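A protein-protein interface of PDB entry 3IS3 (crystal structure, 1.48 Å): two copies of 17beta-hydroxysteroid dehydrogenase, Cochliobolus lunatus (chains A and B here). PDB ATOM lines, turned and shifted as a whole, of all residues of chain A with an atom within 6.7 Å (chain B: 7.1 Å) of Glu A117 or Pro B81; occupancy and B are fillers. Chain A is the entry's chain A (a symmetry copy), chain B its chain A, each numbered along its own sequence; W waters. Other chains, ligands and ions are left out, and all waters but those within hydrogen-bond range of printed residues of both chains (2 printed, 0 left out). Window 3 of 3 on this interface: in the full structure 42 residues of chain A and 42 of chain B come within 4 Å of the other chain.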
ATOM      1  N   VAL A 115       7.917 -34.148  13.910  1.00  0.00           N
ATOM      2  CA  VAL A 115       8.813 -32.998  13.959  1.00  0.00           C
ATOM      3  C   VAL A 115       8.489 -32.126  15.157  1.00  0.00           C
ATOM      4  O   VAL A 115       7.337 -31.777  15.360  1.00  0.00           O
ATOM      5  CB  VAL A 115       8.797 -32.187  12.658  1.00  0.00           C
ATOM      6  CG1 VAL A 115       9.741 -30.959  12.764  1.00  0.00           C
ATOM      7  CG2 VAL A 115       9.212 -33.106  11.474  1.00  0.00           C
ATOM      8  N   THR A 116       9.504 -31.850  15.976  1.00  0.00           N
ATOM      9  CA  THR A 116       9.319 -31.061  17.200  1.00  0.00           C
ATOM     10  C   THR A 116       9.602 -29.581  16.934  1.00  0.00           C
ATOM     11  O   THR A 116      10.279 -29.208  15.968  1.00  0.00           O
ATOM     12  CB  THR A 116      10.277 -31.522  18.326  1.00  0.00           C
ATOM     13  OG1 THR A 116      11.624 -31.303  17.889  1.00  0.00           O
ATOM     14  CG2 THR A 116      10.050 -32.997  18.677  1.00  0.00           C
ATOM     15  N   GLU A 117       9.117 -28.731  17.855  1.00  0.00           N
ATOM     16  CA  GLU A 117       9.547 -27.322  17.882  1.00  0.00           C
ATOM     17  C   GLU A 117      11.058 -27.184  17.859  1.00  0.00           C
ATOM     18  O   GLU A 117      11.582 -26.369  17.114  1.00  0.00           O
ATOM     19  CB  GLU A 117       9.065 -26.669  19.194  1.00  0.00           C
ATOM     20  CG  GLU A 117       7.591 -26.408  19.206  1.00  0.00           C
ATOM     21  CD  GLU A 117       7.233 -25.444  20.294  1.00  0.00           C
ATOM     22  OE1 GLU A 117       7.731 -24.335  20.246  1.00  0.00           O
ATOM     23  OE2 GLU A 117       6.436 -25.799  21.191  1.00  0.00           O
ATOM     24  N   GLU A 118      11.736 -27.968  18.696  1.00  0.00           N
ATOM     25  CA  GLU A 118      13.183 -27.858  18.809  1.00  0.00           C
ATOM     26  C   GLU A 118      13.872 -28.202  17.505  1.00  0.00           C
ATOM     27  O   GLU A 118      14.824 -27.553  17.122  1.00  0.00           O
ATOM     28  CB  GLU A 118      13.701 -28.738  19.943  1.00  0.00           C
ATOM     29  CG  GLU A 118      13.244 -28.257  21.328  1.00  0.00           C
ATOM     30  CD  GLU A 118      11.839 -28.752  21.783  1.00  0.00           C
ATOM     31  OE1 GLU A 118      11.177 -29.372  20.916  1.00  0.00           O
ATOM     32  OE2 GLU A 118      11.347 -28.541  22.928  1.00  0.00           O
ATOM     33  N   GLU A 119      13.378 -29.230  16.807  1.00  0.00           N
ATOM     34  CA  GLU A 119      14.019 -29.631  15.563  1.00  0.00           C
ATOM     35  C   GLU A 119      13.760 -28.584  14.476  1.00  0.00           C
ATOM     36  O   GLU A 119      14.651 -28.218  13.732  1.00  0.00           O
ATOM     37  CB  GLU A 119      13.538 -31.022  15.131  1.00  0.00           C
ATOM     38  CG  GLU A 119      14.245 -31.568  13.863  1.00  0.00           C
ATOM     39  CD  GLU A 119      15.767 -31.810  14.036  1.00  0.00           C
ATOM     40  OE1 GLU A 119      16.244 -31.621  15.169  1.00  0.00           O
ATOM     41  OE2 GLU A 119      16.487 -32.140  13.068  1.00  0.00           O
ATOM     42  N   PHE A 120      12.532 -28.064  14.406  1.00  0.00           N
ATOM     43  CA  PHE A 120      12.242 -27.000  13.464  1.00  0.00           C
ATOM     44  C   PHE A 120      13.247 -25.850  13.642  1.00  0.00           C
ATOM     45  O   PHE A 120      13.859 -25.348  12.674  1.00  0.00           O
ATOM     46  CB  PHE A 120      10.768 -26.502  13.637  1.00  0.00           C
ATOM     47  CG  PHE A 120      10.386 -25.484  12.616  1.00  0.00           C
ATOM     48  CD1 PHE A 120      10.914 -24.192  12.672  1.00  0.00           C
ATOM     49  CD2 PHE A 120       9.578 -25.835  11.548  1.00  0.00           C
ATOM     50  CE1 PHE A 120      10.641 -23.224  11.683  1.00  0.00           C
ATOM     51  CE2 PHE A 120       9.260 -24.855  10.539  1.00  0.00           C
ATOM     52  CZ  PHE A 120       9.785 -23.576  10.594  1.00  0.00           C
ATOM     53  N   ASP A 121      13.389 -25.421  14.905  1.00  0.00           N
ATOM     54  CA  ASP A 121      14.263 -24.268  15.197  1.00  0.00           C
ATOM     55  C   ASP A 121      15.733 -24.560  14.931  1.00  0.00           C
ATOM     56  O   ASP A 121      16.425 -23.700  14.408  1.00  0.00           O
ATOM     57  CB  ASP A 121      14.034 -23.767  16.619  1.00  0.00           C
ATOM     58  CG  ASP A 121      12.619 -23.186  16.809  1.00  0.00           C
ATOM     59  OD1 ASP A 121      12.018 -22.814  15.777  1.00  0.00           O
ATOM     60  OD2 ASP A 121      12.150 -23.089  17.964  1.00  0.00           O
ATOM     61  N   ARG A 122      16.161 -25.790  15.244  1.00  0.00           N
ATOM     62  CA  ARG A 122      17.538 -26.232  14.940  1.00  0.00           C
ATOM     63  C   ARG A 122      17.864 -26.054  13.458  1.00  0.00           C
ATOM     64  O   ARG A 122      18.900 -25.506  13.090  1.00  0.00           O
ATOM     65  CB  ARG A 122      17.758 -27.695  15.331  1.00  0.00           C
ATOM     66  CG  ARG A 122      19.246 -28.094  15.241  1.00  0.00           C
ATOM     67  CD  ARG A 122      19.444 -29.557  15.604  1.00  0.00           C
ATOM     68  NE  ARG A 122      18.918 -30.458  14.581  1.00  0.00           N
ATOM     69  CZ  ARG A 122      19.628 -30.890  13.538  1.00  0.00           C
ATOM     70  NH1 ARG A 122      20.882 -30.489  13.375  1.00  0.00           N
ATOM     71  NH2 ARG A 122      19.072 -31.725  12.667  1.00  0.00           N
ATOM     72  N   ASP B  76      -3.288 -18.409  19.237  1.00  0.00           N
ATOM     73  CA  ASP B  76      -2.059 -17.766  18.777  1.00  0.00           C
ATOM     74  C   ASP B  76      -1.262 -18.839  18.049  1.00  0.00           C
ATOM     75  O   ASP B  76      -0.614 -19.689  18.683  1.00  0.00           O
ATOM     76  CB  ASP B  76      -1.286 -17.172  19.953  1.00  0.00           C
ATOM     77  CG  ASP B  76       0.008 -16.509  19.534  1.00  0.00           C
ATOM     78  OD1 ASP B  76       0.339 -16.554  18.322  1.00  0.00           O
ATOM     79  OD2 ASP B  76       0.685 -15.944  20.430  1.00  0.00           O
ATOM     80  N   ARG B  78       1.403 -18.699  16.480  1.00  0.00           N
ATOM     81  CA  ARG B  78       2.828 -18.710  16.818  1.00  0.00           C
ATOM     82  C   ARG B  78       3.201 -19.659  17.942  1.00  0.00           C
ATOM     83  O   ARG B  78       4.369 -20.020  18.066  1.00  0.00           O
ATOM     84  CB  ARG B  78       3.380 -17.313  17.126  1.00  0.00           C
ATOM     85  CG  ARG B  78       3.344 -16.369  15.917  1.00  0.00           C
ATOM     86  CD  ARG B  78       3.972 -15.043  16.329  1.00  0.00           C
ATOM     87  NE  ARG B  78       4.173 -14.205  15.135  1.00  0.00           N
ATOM     88  CZ  ARG B  78       3.334 -13.272  14.689  1.00  0.00           C
ATOM     89  NH1 ARG B  78       2.209 -13.002  15.341  1.00  0.00           N
ATOM     90  NH2 ARG B  78       3.652 -12.579  13.610  1.00  0.00           N
ATOM     91  N   GLN B  79       2.247 -20.008  18.807  1.00  0.00           N
ATOM     92  CA  GLN B  79       2.517 -20.872  19.942  1.00  0.00           C
ATOM     93  C   GLN B  79       2.035 -22.280  19.629  1.00  0.00           C
ATOM     94  O   GLN B  79       0.821 -22.567  19.606  1.00  0.00           O
ATOM     95  CB  GLN B  79       1.787 -20.341  21.168  1.00  0.00           C
ATOM     96  CG  GLN B  79       2.375 -19.006  21.611  1.00  0.00           C
ATOM     97  CD  GLN B  79       1.794 -18.567  22.928  1.00  0.00           C
ATOM     98  OE1 GLN B  79       1.845 -19.297  23.926  1.00  0.00           O
ATOM     99  NE2 GLN B  79       1.216 -17.363  22.953  1.00  0.00           N
ATOM    100  N   VAL B  80       2.983 -23.180  19.366  1.00  0.00           N
ATOM    101  CA  VAL B  80       2.606 -24.561  19.016  1.00  0.00           C
ATOM    102  C   VAL B  80       1.661 -25.237  20.042  1.00  0.00           C
ATOM    103  O   VAL B  80       0.723 -25.910  19.638  1.00  0.00           O
ATOM    104  CB  VAL B  80       3.874 -25.411  18.712  1.00  0.00           C
ATOM    105  CG1 VAL B  80       3.495 -26.878  18.481  1.00  0.00           C
ATOM    106  CG2 VAL B  80       4.585 -24.857  17.486  1.00  0.00           C
ATOM    107  N   PRO B  81       1.869 -25.052  21.372  1.00  0.00           N
ATOM    108  CA  PRO B  81       0.898 -25.628  22.331  1.00  0.00           C
ATOM    109  C   PRO B  81      -0.549 -25.159  22.096  1.00  0.00           C
ATOM    110  O   PRO B  81      -1.521 -25.902  22.399  1.00  0.00           O
ATOM    111  CB  PRO B  81       1.395 -25.148  23.693  1.00  0.00           C
ATOM    112  CG  PRO B  81       2.760 -24.644  23.479  1.00  0.00           C
ATOM    113  CD  PRO B  81       3.059 -24.475  22.041  1.00  0.00           C
ATOM    114  N   GLU B  82      -0.709 -23.935  21.592  1.00  0.00           N
ATOM    115  CA  GLU B  82      -2.048 -23.435  21.255  1.00  0.00           C
ATOM    116  C   GLU B  82      -2.618 -24.063  19.993  1.00  0.00           C
ATOM    117  O   GLU B  82      -3.841 -24.262  19.914  1.00  0.00           O
ATOM    118  CB  GLU B  82      -2.085 -21.894  21.189  1.00  0.00           C
ATOM    119  CG  GLU B  82      -1.719 -21.286  22.507  1.00  0.00           C
ATOM    120  CD  GLU B  82      -2.070 -19.803  22.607  1.00  0.00           C
ATOM    121  OE1 GLU B  82      -3.020 -19.370  21.914  1.00  0.00           O
ATOM    122  OE2 GLU B  82      -1.402 -19.093  23.400  1.00  0.00           O
ATOM    123  N   ILE B  83      -1.752 -24.410  19.027  1.00  0.00           N
ATOM    124  CA  ILE B  83      -2.218 -25.139  17.850  1.00  0.00           C
ATOM    125  C   ILE B  83      -2.699 -26.536  18.276  1.00  0.00           C
ATOM    126  O   ILE B  83      -3.783 -26.976  17.871  1.00  0.00           O
ATOM    127  CB  ILE B  83      -1.108 -25.278  16.809  1.00  0.00           C
ATOM    128  CG1 ILE B  83      -0.534 -23.900  16.437  1.00  0.00           C
ATOM    129  CG2 ILE B  83      -1.653 -25.972  15.539  1.00  0.00           C
ATOM    130  CD1 ILE B  83       0.727 -24.019  15.548  1.00  0.00           C
ATOM    131  N   VAL B  84      -1.921 -27.200  19.133  1.00  0.00           N
ATOM    132  CA  VAL B  84      -2.341 -28.491  19.694  1.00  0.00           C
ATOM    133  C   VAL B  84      -3.723 -28.382  20.360  1.00  0.00           C
ATOM    134  O   VAL B  84      -4.643 -29.183  20.094  1.00  0.00           O
ATOM    135  CB  VAL B  84      -1.335 -29.039  20.703  1.00  0.00           C
ATOM    136  CG1 VAL B  84      -1.888 -30.311  21.361  1.00  0.00           C
ATOM    137  CG2 VAL B  84       0.001 -29.337  20.030  1.00  0.00           C
ATOM    138  N   LYS B  85      -3.889 -27.392  21.237  1.00  0.00           N
ATOM    139  CA  LYS B  85      -5.175 -27.233  21.920  1.00  0.00           C
ATOM    140  C   LYS B  85      -6.332 -26.905  20.972  1.00  0.00           C
ATOM    141  O   LYS B  85      -7.446 -27.417  21.146  1.00  0.00           O
ATOM    142  CB  LYS B  85      -5.082 -26.178  23.014  1.00  0.00           C
ATOM    143  CG  LYS B  85      -4.266 -26.626  24.212  1.00  0.00           C
ATOM    144  CD  LYS B  85      -4.432 -25.648  25.374  1.00  0.00           C
ATOM    145  CE  LYS B  85      -3.625 -26.103  26.583  1.00  0.00           C
ATOM    146  NZ  LYS B  85      -3.770 -25.150  27.713  1.00  0.00           N
ATOM    147  N   LEU B  86      -6.076 -26.053  19.985  1.00  0.00           N
ATOM    148  CA  LEU B  86      -7.079 -25.721  18.972  1.00  0.00           C
ATOM    149  C   LEU B  86      -7.598 -26.984  18.289  1.00  0.00           C
ATOM    150  O   LEU B  86      -8.809 -27.177  18.174  1.00  0.00           O
ATOM    151  CB  LEU B  86      -6.502 -24.746  17.940  1.00  0.00           C
ATOM    152  CG  LEU B  86      -7.261 -24.600  16.617  1.00  0.00           C
ATOM    153  CD1 LEU B  86      -8.623 -23.940  16.851  1.00  0.00           C
ATOM    154  CD2 LEU B  86      -6.411 -23.787  15.627  1.00  0.00           C
ATOM    155  N   ASP B  88      -7.282 -30.206  19.311  1.00  0.00           N
ATOM    156  CA  ASP B  88      -7.963 -31.042  20.305  1.00  0.00           C
ATOM    157  C   ASP B  88      -9.399 -30.574  20.533  1.00  0.00           C
ATOM    158  O   ASP B  88     -10.342 -31.384  20.637  1.00  0.00           O
ATOM    159  CB  ASP B  88      -7.223 -30.963  21.642  1.00  0.00           C
ATOM    160  CG  ASP B  88      -5.926 -31.781  21.678  1.00  0.00           C
ATOM    161  OD1 ASP B  88      -5.661 -32.620  20.788  1.00  0.00           O
ATOM    162  OD2 ASP B  88      -5.174 -31.581  22.646  1.00  0.00           O
ATOM    163  N   ARG B 129       6.793 -21.237  10.353  1.00  0.00           N
ATOM    164  CA  ARG B 129       6.740 -22.145  11.504  1.00  0.00           C
ATOM    165  C   ARG B 129       5.300 -22.430  11.923  1.00  0.00           C
ATOM    166  O   ARG B 129       4.903 -23.592  12.091  1.00  0.00           O
ATOM    167  CB  ARG B 129       7.547 -21.537  12.649  1.00  0.00           C
ATOM    168  CG  ARG B 129       7.843 -22.511  13.810  1.00  0.00           C
ATOM    169  CD  ARG B 129       8.745 -21.718  14.757  1.00  0.00           C
ATOM    170  NE  ARG B 129       9.246 -22.453  15.910  1.00  0.00           N
ATOM    171  CZ  ARG B 129       8.542 -22.702  17.018  1.00  0.00           C
ATOM    172  NH1 ARG B 129       7.258 -22.328  17.155  1.00  0.00           N
ATOM    173  NH2 ARG B 129       9.162 -23.334  18.015  1.00  0.00           N
ATOM    174  N   PHE B 133       3.351 -26.167  11.745  1.00  0.00           N
ATOM    175  CA  PHE B 133       2.743 -26.893  12.852  1.00  0.00           C
ATOM    176  C   PHE B 133       1.218 -27.012  12.810  1.00  0.00           C
ATOM    177  O   PHE B 133       0.672 -27.970  13.395  1.00  0.00           O
ATOM    178  CB  PHE B 133       3.264 -26.341  14.184  1.00  0.00           C
ATOM    179  CG  PHE B 133       4.697 -26.746  14.443  1.00  0.00           C
ATOM    180  CD1 PHE B 133       5.013 -28.069  14.763  1.00  0.00           C
ATOM    181  CD2 PHE B 133       5.739 -25.832  14.254  1.00  0.00           C
ATOM    182  CE1 PHE B 133       6.322 -28.473  14.963  1.00  0.00           C
ATOM    183  CE2 PHE B 133       7.096 -26.219  14.457  1.00  0.00           C
ATOM    184  CZ  PHE B 133       7.380 -27.558  14.800  1.00  0.00           C
ATOM    185  N   ARG B 136       1.187 -30.099  10.924  1.00  0.00           N
ATOM    186  CA  ARG B 136       1.487 -31.237  11.795  1.00  0.00           C
ATOM    187  C   ARG B 136       0.275 -31.658  12.626  1.00  0.00           C
ATOM    188  O   ARG B 136      -0.061 -32.863  12.718  1.00  0.00           O
ATOM    189  CB  ARG B 136       2.630 -30.903  12.747  1.00  0.00           C
ATOM    190  CG  ARG B 136       3.121 -32.150  13.486  1.00  0.00           C
ATOM    191  CD  ARG B 136       4.038 -31.786  14.622  1.00  0.00           C
ATOM    192  NE  ARG B 136       3.282 -31.244  15.780  1.00  0.00           N
ATOM    193  CZ  ARG B 136       3.851 -30.891  16.930  1.00  0.00           C
ATOM    194  NH1 ARG B 136       5.170 -30.978  17.101  1.00  0.00           N
ATOM    195  NH2 ARG B 136       3.094 -30.418  17.920  1.00  0.00           N
HETATM  196  O   HOH W   1       5.758 -22.522  19.784  1.00  0.00           O
HETATM  197  O   HOH W   2       6.956 -30.155  19.608  1.00  0.00           O
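O of Val A115 touches CE1 of Phe B133 (3.5 Å). Phe B133 touches Thr A116 (CZ to O, 3.5 Å). OE2 of Glu A117 touches CB of Val B80, at 3.6 Å. CD of Pro B81 touches OE2 of Glu A117, 3.7 Å away. Glu A117 touches Phe B133 (N to CZ, 3.7 Å). Phe A120 touches Arg B129. Phe B133 touches Phe A120.
Hydrophobic or aromatic side chains of chain A that line the printed part of chain B: Phe A120. Among the printed residues, 10 pairs touch across the chains.
Of chain B, only Val B80, Pro B81, Arg B129 and Phe B133 come within 4 Å of Glu A117. Printed residues of chain A within 4 Å of Pro B81: Glu A117. Printed residues of chain B within 4 Å of Phe A120: Arg B129 and Phe B133. Of the printed residues of chain A, Arg B129 touches Glu A117, Phe A120 and Asp A121. Asp B88 touches none of the printed residues of chain A. The nearest residue of chain B that does not touch Glu A117 is Arg B136 (4.6 Å). The nearest printed residue of chain A that does not touch Pro B81 is Glu A118 (9.3 Å). The nearest printed residue of chain B that does not touch Phe A120 is Val B80 (7.5 Å).
The side-chain hydroxyl (OG1) of Thr A116 lies within hydrogen-bond range of the backbone NH (N) of Glu A119, 2.9 Å away. The side-chain hydroxyl (OG1) of Thr A116 lies close to the backbone NH (N) of Glu A118, at 3.4 Å.
Water W1 lies within hydrogen-bond range of OE1 of Glu A117, N of Val B80, NH1 of Arg B129 and O of Arg B78. Water W2 lies within hydrogen-bond range of the backbone NH (N) of Glu A117 (3.1 Å) and the guanidinium group (NH1) of Arg B136 (3.2 Å).
NE of Arg B129 is in salt-bridge range of OD1 of Asp A121 (2.8 Å). The guanidinium group of Arg B136 sits at hydrogen-bond distance from the backbone carbonyl oxygen of Val A115 (2.9 Å). The guanidinium group of Arg B129 lies within salt-bridge range of the side-chain carboxylate of Glu A117, 2.8 Å away.
No position is printed for both chains. Of the 10 pairs that touch across the chains among the printed residues, none has its exchanged pair printed and touching as well.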
